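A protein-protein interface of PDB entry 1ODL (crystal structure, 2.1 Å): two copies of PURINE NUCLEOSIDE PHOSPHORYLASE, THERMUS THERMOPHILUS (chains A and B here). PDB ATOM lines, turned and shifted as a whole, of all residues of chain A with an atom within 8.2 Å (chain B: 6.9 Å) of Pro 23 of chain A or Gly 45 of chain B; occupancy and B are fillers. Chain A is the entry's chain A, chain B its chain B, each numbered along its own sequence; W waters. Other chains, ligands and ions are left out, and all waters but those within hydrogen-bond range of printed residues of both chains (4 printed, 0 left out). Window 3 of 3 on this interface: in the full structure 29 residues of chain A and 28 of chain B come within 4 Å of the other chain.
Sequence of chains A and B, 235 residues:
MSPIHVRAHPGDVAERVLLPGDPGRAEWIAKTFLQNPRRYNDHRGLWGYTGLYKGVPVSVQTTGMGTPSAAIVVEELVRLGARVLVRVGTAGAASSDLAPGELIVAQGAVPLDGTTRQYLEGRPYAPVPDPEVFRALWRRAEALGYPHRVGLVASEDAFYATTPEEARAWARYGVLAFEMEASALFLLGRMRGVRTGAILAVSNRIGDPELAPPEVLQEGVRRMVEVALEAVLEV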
ATOM      1  N   PRO A  20     -18.461 -19.087  13.756  1.00  0.00           N
ATOM      2  CA  PRO A  20     -17.802 -18.020  12.991  1.00  0.00           C
ATOM      3  C   PRO A  20     -16.297 -18.169  13.226  1.00  0.00           C
ATOM      4  O   PRO A  20     -15.881 -18.667  14.277  1.00  0.00           O
ATOM      5  CB  PRO A  20     -18.365 -16.750  13.626  1.00  0.00           C
ATOM      6  CG  PRO A  20     -18.530 -17.154  15.071  1.00  0.00           C
ATOM      7  CD  PRO A  20     -19.140 -18.545  14.950  1.00  0.00           C
ATOM      8  N   GLY A  21     -15.480 -17.753  12.264  1.00  0.00           N
ATOM      9  CA  GLY A  21     -14.038 -17.869  12.442  1.00  0.00           C
ATOM     10  C   GLY A  21     -13.453 -16.726  13.259  1.00  0.00           C
ATOM     11  O   GLY A  21     -12.472 -16.897  13.990  1.00  0.00           O
ATOM     12  N   ASP A  22     -14.077 -15.558  13.134  1.00  0.00           N
ATOM     13  CA  ASP A  22     -13.659 -14.339  13.817  1.00  0.00           C
ATOM     14  C   ASP A  22     -14.400 -14.132  15.146  1.00  0.00           C
ATOM     15  O   ASP A  22     -15.629 -14.149  15.186  1.00  0.00           O
ATOM     16  CB  ASP A  22     -13.909 -13.153  12.876  1.00  0.00           C
ATOM     17  CG  ASP A  22     -13.552 -11.809  13.494  1.00  0.00           C
ATOM     18  OD1 ASP A  22     -13.021 -11.755  14.625  1.00  0.00           O
ATOM     19  OD2 ASP A  22     -13.807 -10.791  12.825  1.00  0.00           O
ATOM     20  N   PRO A  23     -13.653 -13.947  16.253  1.00  0.00           N
ATOM     21  CA  PRO A  23     -14.257 -13.736  17.572  1.00  0.00           C
ATOM     22  C   PRO A  23     -15.090 -12.460  17.599  1.00  0.00           C
ATOM     23  O   PRO A  23     -16.059 -12.361  18.350  1.00  0.00           O
ATOM     24  CB  PRO A  23     -13.044 -13.673  18.508  1.00  0.00           C
ATOM     25  CG  PRO A  23     -11.945 -13.147  17.615  1.00  0.00           C
ATOM     26  CD  PRO A  23     -12.178 -13.931  16.344  1.00  0.00           C
ATOM     27  N   GLY A  24     -14.716 -11.494  16.766  1.00  0.00           N
ATOM     28  CA  GLY A  24     -15.458 -10.245  16.706  1.00  0.00           C
ATOM     29  C   GLY A  24     -16.864 -10.464  16.174  1.00  0.00           C
ATOM     30  O   GLY A  24     -17.825  -9.863  16.657  1.00  0.00           O
ATOM     31  N   ARG A  25     -16.992 -11.338  15.182  1.00  0.00           N
ATOM     32  CA  ARG A  25     -18.297 -11.628  14.606  1.00  0.00           C
ATOM     33  C   ARG A  25     -19.129 -12.459  15.572  1.00  0.00           C
ATOM     34  O   ARG A  25     -20.356 -12.342  15.608  1.00  0.00           O
ATOM     35  CB  ARG A  25     -18.154 -12.382  13.284  1.00  0.00           C
ATOM     36  CG  ARG A  25     -19.489 -12.579  12.569  1.00  0.00           C
ATOM     37  CD  ARG A  25     -19.320 -13.309  11.256  1.00  0.00           C
ATOM     38  NE  ARG A  25     -18.249 -12.715  10.469  1.00  0.00           N
ATOM     39  CZ  ARG A  25     -17.194 -13.391  10.035  1.00  0.00           C
ATOM     40  NH1 ARG A  25     -17.082 -14.685  10.306  1.00  0.00           N
ATOM     41  NH2 ARG A  25     -16.239 -12.768   9.356  1.00  0.00           N
ATOM     42  N   ALA A  26     -18.457 -13.315  16.337  1.00  0.00           N
ATOM     43  CA  ALA A  26     -19.144 -14.153  17.314  1.00  0.00           C
ATOM     44  C   ALA A  26     -19.800 -13.228  18.332  1.00  0.00           C
ATOM     45  O   ALA A  26     -20.980 -13.381  18.656  1.00  0.00           O
ATOM     46  CB  ALA A  26     -18.159 -15.079  18.006  1.00  0.00           C
ATOM     47  N   GLU A  27     -19.028 -12.265  18.833  1.00  0.00           N
ATOM     48  CA  GLU A  27     -19.553 -11.307  19.791  1.00  0.00           C
ATOM     49  C   GLU A  27     -20.687 -10.505  19.166  1.00  0.00           C
ATOM     50  O   GLU A  27     -21.704 -10.257  19.813  1.00  0.00           O
ATOM     51  CB  GLU A  27     -18.462 -10.339  20.249  1.00  0.00           C
ATOM     52  CG  GLU A  27     -18.989  -9.226  21.154  1.00  0.00           C
ATOM     53  CD  GLU A  27     -17.900  -8.283  21.626  1.00  0.00           C
ATOM     54  OE1 GLU A  27     -17.198  -7.702  20.769  1.00  0.00           O
ATOM     55  OE2 GLU A  27     -17.748  -8.123  22.857  1.00  0.00           O
ATOM     56  N   TRP A  28     -20.506 -10.092  17.913  1.00  0.00           N
ATOM     57  CA  TRP A  28     -21.527  -9.311  17.223  1.00  0.00           C
ATOM     58  C   TRP A  28     -22.815 -10.114  17.030  1.00  0.00           C
ATOM     59  O   TRP A  28     -23.919  -9.575  17.152  1.00  0.00           O
ATOM     60  CB  TRP A  28     -21.011  -8.836  15.862  1.00  0.00           C
ATOM     61  CG  TRP A  28     -22.020  -8.040  15.096  1.00  0.00           C
ATOM     62  CD1 TRP A  28     -22.364  -6.731  15.301  1.00  0.00           C
ATOM     63  CD2 TRP A  28     -22.871  -8.519  14.047  1.00  0.00           C
ATOM     64  NE1 TRP A  28     -23.379  -6.368  14.445  1.00  0.00           N
ATOM     65  CE2 TRP A  28     -23.712  -7.447  13.667  1.00  0.00           C
ATOM     66  CE3 TRP A  28     -23.009  -9.753  13.393  1.00  0.00           C
ATOM     67  CZ2 TRP A  28     -24.679  -7.572  12.660  1.00  0.00           C
ATOM     68  CZ3 TRP A  28     -23.971  -9.879  12.391  1.00  0.00           C
ATOM     69  CH2 TRP A  28     -24.793  -8.792  12.036  1.00  0.00           C
ATOM     70  N   ILE A  29     -22.667 -11.399  16.724  1.00  0.00           N
ATOM     71  CA  ILE A  29     -23.818 -12.277  16.523  1.00  0.00           C
ATOM     72  C   ILE A  29     -24.612 -12.444  17.820  1.00  0.00           C
ATOM     73  O   ILE A  29     -25.836 -12.305  17.831  1.00  0.00           O
ATOM     74  CB  ILE A  29     -23.371 -13.675  16.023  1.00  0.00           C
ATOM     75  CG1 ILE A  29     -22.817 -13.572  14.603  1.00  0.00           C
ATOM     76  CG2 ILE A  29     -24.542 -14.650  16.047  1.00  0.00           C
ATOM     77  CD1 ILE A  29     -22.120 -14.846  14.144  1.00  0.00           C
ATOM     78  N   ALA A  30     -23.911 -12.734  18.911  1.00  0.00           N
ATOM     79  CA  ALA A  30     -24.557 -12.931  20.206  1.00  0.00           C
ATOM     80  C   ALA A  30     -25.357 -11.711  20.635  1.00  0.00           C
ATOM     81  O   ALA A  30     -26.518 -11.825  21.025  1.00  0.00           O
ATOM     82  CB  ALA A  30     -23.522 -13.257  21.261  1.00  0.00           C
ATOM     83  N   ARG A  39     -21.111 -15.224  27.692  1.00  0.00           N
ATOM     84  CA  ARG A  39     -19.842 -15.752  27.194  1.00  0.00           C
ATOM     85  C   ARG A  39     -19.321 -16.830  28.131  1.00  0.00           C
ATOM     86  O   ARG A  39     -18.936 -16.533  29.261  1.00  0.00           O
ATOM     87  CB  ARG A  39     -18.800 -14.631  27.079  1.00  0.00           C
ATOM     88  CG  ARG A  39     -17.498 -15.089  26.457  1.00  0.00           C
ATOM     89  CD  ARG A  39     -16.633 -13.926  26.000  1.00  0.00           C
ATOM     90  NE  ARG A  39     -15.980 -13.241  27.111  1.00  0.00           N
ATOM     91  CZ  ARG A  39     -15.172 -12.196  26.969  1.00  0.00           C
ATOM     92  NH1 ARG A  39     -14.915 -11.707  25.763  1.00  0.00           N
ATOM     93  NH2 ARG A  39     -14.608 -11.648  28.032  1.00  0.00           N
ATOM     94  N   ASN A  41     -16.707 -18.873  27.337  1.00  0.00           N
ATOM     95  CA  ASN A  41     -15.275 -19.063  27.136  1.00  0.00           C
ATOM     96  C   ASN A  41     -14.584 -17.909  26.446  1.00  0.00           C
ATOM     97  O   ASN A  41     -15.131 -17.297  25.528  1.00  0.00           O
ATOM     98  CB  ASN A  41     -14.987 -20.309  26.300  1.00  0.00           C
ATOM     99  CG  ASN A  41     -13.489 -20.537  26.104  1.00  0.00           C
ATOM    100  OD1 ASN A  41     -12.795 -20.974  27.020  1.00  0.00           O
ATOM    101  ND2 ASN A  41     -12.985 -20.222  24.914  1.00  0.00           N
ATOM    102  N   ARG A  44      -7.770 -18.487  25.012  1.00  0.00           N
ATOM    103  CA  ARG A  44      -7.132 -18.451  23.700  1.00  0.00           C
ATOM    104  C   ARG A  44      -7.832 -17.536  22.699  1.00  0.00           C
ATOM    105  O   ARG A  44      -7.514 -17.537  21.506  1.00  0.00           O
ATOM    106  CB  ARG A  44      -6.996 -19.871  23.130  1.00  0.00           C
ATOM    107  CG  ARG A  44      -5.733 -20.609  23.615  1.00  0.00           C
ATOM    108  CD  ARG A  44      -5.621 -22.020  23.028  1.00  0.00           C
ATOM    109  NE  ARG A  44      -4.426 -22.723  23.498  1.00  0.00           N
ATOM    110  CZ  ARG A  44      -3.199 -22.552  23.006  1.00  0.00           C
ATOM    111  NH1 ARG A  44      -2.983 -21.704  22.012  1.00  0.00           N
ATOM    112  NH2 ARG A  44      -2.177 -23.218  23.523  1.00  0.00           N
ATOM    113  N   GLY A  45      -8.763 -16.728  23.192  1.00  0.00           N
ATOM    114  CA  GLY A  45      -9.487 -15.822  22.313  1.00  0.00           C
ATOM    115  C   GLY A  45     -10.591 -16.518  21.534  1.00  0.00           C
ATOM    116  O   GLY A  45     -11.193 -15.930  20.636  1.00  0.00           O
ATOM    117  N   LEU A  46     -10.865 -17.773  21.875  1.00  0.00           N
ATOM    118  CA  LEU A  46     -11.912 -18.527  21.192  1.00  0.00           C
ATOM    119  C   LEU A  46     -13.250 -18.203  21.859  1.00  0.00           C
ATOM    120  O   LEU A  46     -13.894 -19.065  22.458  1.00  0.00           O
ATOM    121  CB  LEU A  46     -11.603 -20.026  21.273  1.00  0.00           C
ATOM    122  CG  LEU A  46     -10.241 -20.464  20.699  1.00  0.00           C
ATOM    123  CD1 LEU A  46      -9.930 -21.889  21.139  1.00  0.00           C
ATOM    124  CD2 LEU A  46     -10.249 -20.370  19.177  1.00  0.00           C
ATOM    125  N   TRP A  47     -13.657 -16.940  21.755  1.00  0.00           N
ATOM    126  CA  TRP A  47     -14.904 -16.484  22.364  1.00  0.00           C
ATOM    127  C   TRP A  47     -16.109 -17.338  21.974  1.00  0.00           C
ATOM    128  O   TRP A  47     -16.395 -17.533  20.787  1.00  0.00           O
ATOM    129  CB  TRP A  47     -15.170 -15.020  21.997  1.00  0.00           C
ATOM    130  CG  TRP A  47     -14.159 -14.050  22.550  1.00  0.00           C
ATOM    131  CD1 TRP A  47     -13.053 -14.347  23.300  1.00  0.00           C
ATOM    132  CD2 TRP A  47     -14.166 -12.627  22.395  1.00  0.00           C
ATOM    133  NE1 TRP A  47     -12.372 -13.199  23.619  1.00  0.00           N
ATOM    134  CE2 TRP A  47     -13.032 -12.127  23.078  1.00  0.00           C
ATOM    135  CE3 TRP A  47     -15.019 -11.723  21.746  1.00  0.00           C
ATOM    136  CZ2 TRP A  47     -12.730 -10.760  23.129  1.00  0.00           C
ATOM    137  CZ3 TRP A  47     -14.717 -10.363  21.796  1.00  0.00           C
ATOM    138  CH2 TRP A  47     -13.580  -9.897  22.485  1.00  0.00           C
ATOM    139  N   GLY A  48     -16.805 -17.843  22.991  1.00  0.00           N
ATOM    140  CA  GLY A  48     -17.983 -18.662  22.777  1.00  0.00           C
ATOM    141  C   GLY A  48     -19.120 -18.160  23.649  1.00  0.00           C
ATOM    142  O   GLY A  48     -18.928 -17.913  24.839  1.00  0.00           O
ATOM    143  N   TYR A  49     -20.300 -18.010  23.054  1.00  0.00           N
ATOM    144  CA  TYR A  49     -21.473 -17.523  23.771  1.00  0.00           C
ATOM    145  C   TYR A  49     -22.659 -18.467  23.638  1.00  0.00           C
ATOM    146  O   TYR A  49     -22.761 -19.231  22.677  1.00  0.00           O
ATOM    147  CB  TYR A  49     -21.916 -16.159  23.231  1.00  0.00           C
ATOM    148  CG  TYR A  49     -20.830 -15.117  23.122  1.00  0.00           C
ATOM    149  CD1 TYR A  49     -19.864 -15.191  22.118  1.00  0.00           C
ATOM    150  CD2 TYR A  49     -20.769 -14.052  24.019  1.00  0.00           C
ATOM    151  CE1 TYR A  49     -18.864 -14.233  22.010  1.00  0.00           C
ATOM    152  CE2 TYR A  49     -19.770 -13.082  23.920  1.00  0.00           C
ATOM    153  CZ  TYR A  49     -18.823 -13.181  22.913  1.00  0.00           C
ATOM    154  OH  TYR A  49     -17.836 -12.232  22.805  1.00  0.00           O
ATOM    155  N   VAL A  60     -22.704 -19.646  19.878  1.00  0.00           N
ATOM    156  CA  VAL A  60     -21.903 -19.035  18.818  1.00  0.00           C
ATOM    157  C   VAL A  60     -20.460 -19.190  19.288  1.00  0.00           C
ATOM    158  O   VAL A  60     -20.011 -18.460  20.173  1.00  0.00           O
ATOM    159  CB  VAL A  60     -22.230 -17.532  18.652  1.00  0.00           C
ATOM    160  CG1 VAL A  60     -21.405 -16.940  17.514  1.00  0.00           C
ATOM    161  CG2 VAL A  60     -23.718 -17.352  18.386  1.00  0.00           C
ATOM    162  N   GLN A  61     -19.743 -20.147  18.700  1.00  0.00           N
ATOM    163  CA  GLN A  61     -18.363 -20.435  19.094  1.00  0.00           C
ATOM    164  C   GLN A  61     -17.306 -20.095  18.056  1.00  0.00           C
ATOM    165  O   GLN A  61     -17.358 -20.567  16.924  1.00  0.00           O
ATOM    166  CB  GLN A  61     -18.223 -21.917  19.450  1.00  0.00           C
ATOM    167  CG  GLN A  61     -16.790 -22.355  19.761  1.00  0.00           C
ATOM    168  CD  GLN A  61     -16.252 -21.727  21.038  1.00  0.00           C
ATOM    169  OE1 GLN A  61     -16.849 -21.858  22.107  1.00  0.00           O
ATOM    170  NE2 GLN A  61     -15.117 -21.050  20.934  1.00  0.00           N
ATOM    171  N   THR A  62     -16.338 -19.284  18.467  1.00  0.00           N
ATOM    172  CA  THR A  62     -15.238 -18.876  17.599  1.00  0.00           C
ATOM    173  C   THR A  62     -14.370 -20.093  17.259  1.00  0.00           C
ATOM    174  O   THR A  62     -14.008 -20.862  18.146  1.00  0.00           O
ATOM    175  CB  THR A  62     -14.368 -17.826  18.307  1.00  0.00           C
ATOM    176  OG1 THR A  62     -15.153 -16.650  18.562  1.00  0.00           O
ATOM    177  CG2 THR A  62     -13.153 -17.476  17.456  1.00  0.00           C
ATOM    178  N   THR A  63     -14.037 -20.266  15.982  1.00  0.00           N
ATOM    179  CA  THR A  63     -13.210 -21.397  15.563  1.00  0.00           C
ATOM    180  C   THR A  63     -11.768 -21.002  15.298  1.00  0.00           C
ATOM    181  O   THR A  63     -10.874 -21.841  15.356  1.00  0.00           O
ATOM    182  CB  THR A  63     -13.725 -22.056  14.260  1.00  0.00           C
ATOM    183  OG1 THR A  63     -13.742 -21.077  13.214  1.00  0.00           O
ATOM    184  CG2 THR A  63     -15.133 -22.644  14.446  1.00  0.00           C
ATOM    185  N   GLY A  64     -11.540 -19.725  15.011  1.00  0.00           N
ATOM    186  CA  GLY A  64     -10.198 -19.287  14.682  1.00  0.00           C
ATOM    187  C   GLY A  64     -10.058 -19.566  13.194  1.00  0.00           C
ATOM    188  O   GLY A  64     -10.967 -20.144  12.602  1.00  0.00           O
ATOM    189  N   MET A  65      -8.941 -19.173  12.587  1.00  0.00           N
ATOM    190  CA  MET A  65      -8.732 -19.388  11.155  1.00  0.00           C
ATOM    191  C   MET A  65      -7.961 -20.673  10.849  1.00  0.00           C
ATOM    192  O   MET A  65      -6.976 -20.977  11.510  1.00  0.00           O
ATOM    193  CB  MET A  65      -7.971 -18.207  10.551  1.00  0.00           C
ATOM    194  CG  MET A  65      -8.696 -16.873  10.648  1.00  0.00           C
ATOM    195  SD  MET A  65      -7.760 -15.533   9.881  1.00  0.00           S
ATOM    196  CE  MET A  65      -6.436 -15.348  11.050  1.00  0.00           C
ATOM    197  N   GLY B  21       1.233 -18.478  20.415  1.00  0.00           N
ATOM    198  CA  GLY B  21       0.022 -18.836  19.695  1.00  0.00           C
ATOM    199  C   GLY B  21      -1.234 -18.366  20.404  1.00  0.00           C
ATOM    200  O   GLY B  21      -2.252 -18.072  19.770  1.00  0.00           O
ATOM    201  N   ASP B  22      -1.146 -18.288  21.728  1.00  0.00           N
ATOM    202  CA  ASP B  22      -2.250 -17.878  22.600  1.00  0.00           C
ATOM    203  C   ASP B  22      -2.240 -16.367  22.927  1.00  0.00           C
ATOM    204  O   ASP B  22      -1.272 -15.846  23.488  1.00  0.00           O
ATOM    205  CB  ASP B  22      -2.172 -18.736  23.878  1.00  0.00           C
ATOM    206  CG  ASP B  22      -3.150 -18.308  24.952  1.00  0.00           C
ATOM    207  OD1 ASP B  22      -4.063 -17.503  24.678  1.00  0.00           O
ATOM    208  OD2 ASP B  22      -2.997 -18.798  26.090  1.00  0.00           O
ATOM    209  N   PRO B  23      -3.324 -15.646  22.578  1.00  0.00           N
ATOM    210  CA  PRO B  23      -3.415 -14.205  22.843  1.00  0.00           C
ATOM    211  C   PRO B  23      -3.266 -13.835  24.318  1.00  0.00           C
ATOM    212  O   PRO B  23      -2.843 -12.727  24.644  1.00  0.00           O
ATOM    213  CB  PRO B  23      -4.797 -13.834  22.291  1.00  0.00           C
ATOM    214  CG  PRO B  23      -5.583 -15.101  22.485  1.00  0.00           C
ATOM    215  CD  PRO B  23      -4.594 -16.156  22.032  1.00  0.00           C
ATOM    216  N   ASN B  41      -2.939  -4.082  17.729  1.00  0.00           N
ATOM    217  CA  ASN B  41      -3.980  -4.825  17.020  1.00  0.00           C
ATOM    218  C   ASN B  41      -4.732  -5.804  17.896  1.00  0.00           C
ATOM    219  O   ASN B  41      -4.137  -6.488  18.732  1.00  0.00           O
ATOM    220  CB  ASN B  41      -3.389  -5.623  15.857  1.00  0.00           C
ATOM    221  CG  ASN B  41      -4.443  -6.459  15.129  1.00  0.00           C
ATOM    222  OD1 ASN B  41      -5.277  -5.925  14.395  1.00  0.00           O
ATOM    223  ND2 ASN B  41      -4.416  -7.772  15.343  1.00  0.00           N
ATOM    224  N   ASP B  42      -6.045  -5.872  17.699  1.00  0.00           N
ATOM    225  CA  ASP B  42      -6.852  -6.835  18.426  1.00  0.00           C
ATOM    226  C   ASP B  42      -7.882  -7.450  17.480  1.00  0.00           C
ATOM    227  O   ASP B  42      -8.686  -8.286  17.884  1.00  0.00           O
ATOM    228  CB  ASP B  42      -7.530  -6.198  19.652  1.00  0.00           C
ATOM    229  CG  ASP B  42      -8.624  -5.212  19.288  1.00  0.00           C
ATOM    230  OD1 ASP B  42      -9.288  -4.715  20.223  1.00  0.00           O
ATOM    231  OD2 ASP B  42      -8.824  -4.930  18.088  1.00  0.00           O
ATOM    232  N   HIS B  43      -7.843  -7.037  16.213  1.00  0.00           N
ATOM    233  CA  HIS B  43      -8.762  -7.567  15.213  1.00  0.00           C
ATOM    234  C   HIS B  43      -8.612  -9.087  15.135  1.00  0.00           C
ATOM    235  O   HIS B  43      -7.494  -9.608  15.175  1.00  0.00           O
ATOM    236  CB  HIS B  43      -8.479  -6.959  13.839  1.00  0.00           C
ATOM    237  CG  HIS B  43      -9.454  -7.382  12.788  1.00  0.00           C
ATOM    238  ND1 HIS B  43      -9.072  -8.016  11.624  1.00  0.00           N
ATOM    239  CD2 HIS B  43     -10.804  -7.301  12.744  1.00  0.00           C
ATOM    240  CE1 HIS B  43     -10.145  -8.310  10.912  1.00  0.00           C
ATOM    241  NE2 HIS B  43     -11.208  -7.887  11.570  1.00  0.00           N
ATOM    242  N   ARG B  44      -9.739  -9.789  15.023  1.00  0.00           N
ATOM    243  CA  ARG B  44      -9.751 -11.253  14.964  1.00  0.00           C
ATOM    244  C   ARG B  44      -9.066 -11.876  16.180  1.00  0.00           C
ATOM    245  O   ARG B  44      -8.591 -13.008  16.128  1.00  0.00           O
ATOM    246  CB  ARG B  44      -9.079 -11.757  13.679  1.00  0.00           C
ATOM    247  CG  ARG B  44     -10.015 -11.823  12.465  1.00  0.00           C
ATOM    248  CD  ARG B  44      -9.291 -12.337  11.220  1.00  0.00           C
ATOM    249  NE  ARG B  44     -10.172 -12.469  10.056  1.00  0.00           N
ATOM    250  CZ  ARG B  44     -11.065 -13.444   9.883  1.00  0.00           C
ATOM    251  NH1 ARG B  44     -11.211 -14.392  10.799  1.00  0.00           N
ATOM    252  NH2 ARG B  44     -11.810 -13.477   8.781  1.00  0.00           N
ATOM    253  N   GLY B  45      -9.022 -11.129  17.276  1.00  0.00           N
ATOM    254  CA  GLY B  45      -8.398 -11.633  18.487  1.00  0.00           C
ATOM    255  C   GLY B  45      -6.911 -11.920  18.353  1.00  0.00           C
ATOM    256  O   GLY B  45      -6.337 -12.646  19.169  1.00  0.00           O
ATOM    257  N   LEU B  46      -6.280 -11.349  17.333  1.00  0.00           N
ATOM    258  CA  LEU B  46      -4.855 -11.559  17.114  1.00  0.00           C
ATOM    259  C   LEU B  46      -4.068 -10.452  17.815  1.00  0.00           C
ATOM    260  O   LEU B  46      -3.362  -9.662  17.184  1.00  0.00           O
ATOM    261  CB  LEU B  46      -4.559 -11.573  15.612  1.00  0.00           C
ATOM    262  CG  LEU B  46      -5.255 -12.680  14.807  1.00  0.00           C
ATOM    263  CD1 LEU B  46      -5.021 -12.469  13.318  1.00  0.00           C
ATOM    264  CD2 LEU B  46      -4.729 -14.043  15.249  1.00  0.00           C
ATOM    265  N   TRP B  47      -4.200 -10.416  19.135  1.00  0.00           N
ATOM    266  CA  TRP B  47      -3.546  -9.419  19.962  1.00  0.00           C
ATOM    267  C   TRP B  47      -2.059  -9.257  19.652  1.00  0.00           C
ATOM    268  O   TRP B  47      -1.284 -10.216  19.698  1.00  0.00           O
ATOM    269  CB  TRP B  47      -3.761  -9.762  21.442  1.00  0.00           C
ATOM    270  CG  TRP B  47      -5.210  -9.695  21.858  1.00  0.00           C
ATOM    271  CD1 TRP B  47      -6.270  -9.355  21.070  1.00  0.00           C
ATOM    272  CD2 TRP B  47      -5.747  -9.951  23.160  1.00  0.00           C
ATOM    273  NE1 TRP B  47      -7.434  -9.380  21.798  1.00  0.00           N
ATOM    274  CE2 TRP B  47      -7.144  -9.741  23.084  1.00  0.00           C
ATOM    275  CE3 TRP B  47      -5.187 -10.334  24.388  1.00  0.00           C
ATOM    276  CZ2 TRP B  47      -7.990  -9.902  24.190  1.00  0.00           C
ATOM    277  CZ3 TRP B  47      -6.031 -10.494  25.489  1.00  0.00           C
ATOM    278  CH2 TRP B  47      -7.415 -10.278  25.380  1.00  0.00           C
ATOM    279  N   GLY B  48      -1.683  -8.027  19.316  1.00  0.00           N
ATOM    280  CA  GLY B  48      -0.302  -7.713  18.993  1.00  0.00           C
ATOM    281  C   GLY B  48       0.148  -6.522  19.813  1.00  0.00           C
ATOM    282  O   GLY B  48      -0.562  -5.514  19.905  1.00  0.00           O
ATOM    283  N   GLN B  61       3.330 -10.854  18.935  1.00  0.00           N
ATOM    284  CA  GLN B  61       2.151 -11.072  18.100  1.00  0.00           C
ATOM    285  C   GLN B  61       1.518 -12.467  18.163  1.00  0.00           C
ATOM    286  O   GLN B  61       2.165 -13.483  17.905  1.00  0.00           O
ATOM    287  CB  GLN B  61       2.490 -10.725  16.645  1.00  0.00           C
ATOM    288  CG  GLN B  61       1.381 -10.994  15.641  1.00  0.00           C
ATOM    289  CD  GLN B  61       0.175 -10.100  15.845  1.00  0.00           C
ATOM    290  OE1 GLN B  61       0.274  -8.875  15.754  1.00  0.00           O
ATOM    291  NE2 GLN B  61      -0.971 -10.706  16.128  1.00  0.00           N
ATOM    292  N   THR B  62       0.233 -12.488  18.501  1.00  0.00           N
ATOM    293  CA  THR B  62      -0.549 -13.719  18.586  1.00  0.00           C
ATOM    294  C   THR B  62      -0.639 -14.315  17.184  1.00  0.00           C
ATOM    295  O   THR B  62      -0.887 -13.588  16.223  1.00  0.00           O
ATOM    296  CB  THR B  62      -1.975 -13.399  19.088  1.00  0.00           C
ATOM    297  OG1 THR B  62      -1.902 -12.865  20.418  1.00  0.00           O
ATOM    298  CG2 THR B  62      -2.851 -14.633  19.070  1.00  0.00           C
ATOM    299  N   GLY B  64      -2.414 -17.462  16.681  1.00  0.00           N
ATOM    300  CA  GLY B  64      -3.579 -18.322  16.608  1.00  0.00           C
ATOM    301  C   GLY B  64      -3.008 -19.730  16.583  1.00  0.00           C
ATOM    302  O   GLY B  64      -1.788 -19.897  16.670  1.00  0.00           O
HETATM  303  O   HOH W   1      -4.562 -19.715  20.395  1.00  0.00           O
HETATM  304  O   HOH W   2     -10.318 -15.322  13.424  1.00  0.00           O
HETATM  305  O   HOH W   3     -12.444  -9.012  14.888  1.00  0.00           O
HETATM  306  O   HOH W   4      -6.092 -17.507  26.928  1.00  0.00           O
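The side-chain sulfur (SD) of Met 65 of chain A lies close to the guanidinium group (NH1) of Arg 44 of chain B.
The side-chain carboxylate (OD1) of Asp 22 of chain A sits at hydrogen-bond distance from the backbone NH (N) of Gly 24 of chain A, at 2.7 Å.
The side-chain amide nitrogen of Asn 41 of chain B sits at hydrogen-bond distance from the backbone carbonyl oxygen of Leu 46 of chain B (2.8 Å).
The backbone carbonyl oxygen of Leu 46 of chain B lies within hydrogen-bond range of the side-chain amide nitrogen of Gln 61 of chain B, 2.8 Å away.
Arg 44 of chain B touches Asp 22 of chain A.
CG of Pro 23 of chain A touches C of Arg 44 of chain B (3.5 Å).
Gly 45 of chain B touches Pro 23 of chain A.
CA of Arg 44 of chain A touches OD1 of Asp 22 of chain B, 3.4 Å away.
CG of Pro 23 of chain B touches O of Arg 44 of chain A, at 3.3 Å.
Gly 45 of chain A touches Pro 23 of chain B (N to CG, 3.6 Å).
CE of Met 65 of chain A touches CD1 of Leu 46 of chain B, 3.9 Å away.
Ile 29 of chain A touches none of the printed residues of chain B.
Of the printed residues of chain B, Gly 45 of chain A touches Pro 23.
Printed residues of chain B within 4 Å of Met 65 of chain A: Arg 44 and Leu 46.
Asn 41 of chain B touches none of the printed residues of chain A.
Of the printed residues of chain A, Arg 44 of chain B touches Asp 22, Pro 23 and Met 65.
Of chain A, only Pro 23 comes within 4 Å of Gly 45 of chain B.
The nearest residue of chain B that does not touch Pro 23 of chain A is His 43 of chain B (5.8 Å).
Hydrophobic or aromatic side chains of chain A within 4 Å of the printed part of chain B: Pro 23 and Met 65.
Printed residues of chain B that touch a printed residue of chain A: Asp 22, Pro 23, Arg 44, Gly 45 and Leu 46.
Hydrophobic or aromatic side chains of chain B that line the printed part of chain A: Pro 23 and Leu 46.
Among the printed residues, 8 pairs touch across the chains.
Among the printed residues, no Asp or Glu carboxylate lies within 4 Å of a Lys or Arg side-chain nitrogen of the other chain.
Asp 22 of chain A touches Arg 44 of chain B, and with the chains exchanged Arg 44 of chain A touches Asp 22 of chain B.
Pro 23 of chain A touches Arg 44 of chain B, and with the chains exchanged Arg 44 of chain A touches Pro 23 of chain B.
Pro 23 of chain A touches Gly 45 of chain B, and with the chains exchanged Gly 45 of chain A touches Pro 23 of chain B.
12 positions are printed for both chains.
Water W2 lies within hydrogen-bond range of O of Gly 21 of chain A (2.7 Å) and NH1 of Arg 44 of chain B (2.9 Å).
Water W3 bridges OD1 of Asp 22 of chain A (2.8 Å) and N of Arg 44 of chain B (2.8 Å).
Water W1 bridges the backbone carbonyl oxygen of Gly 21 of chain B and the guanidinium group of Arg 44 of chain A.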
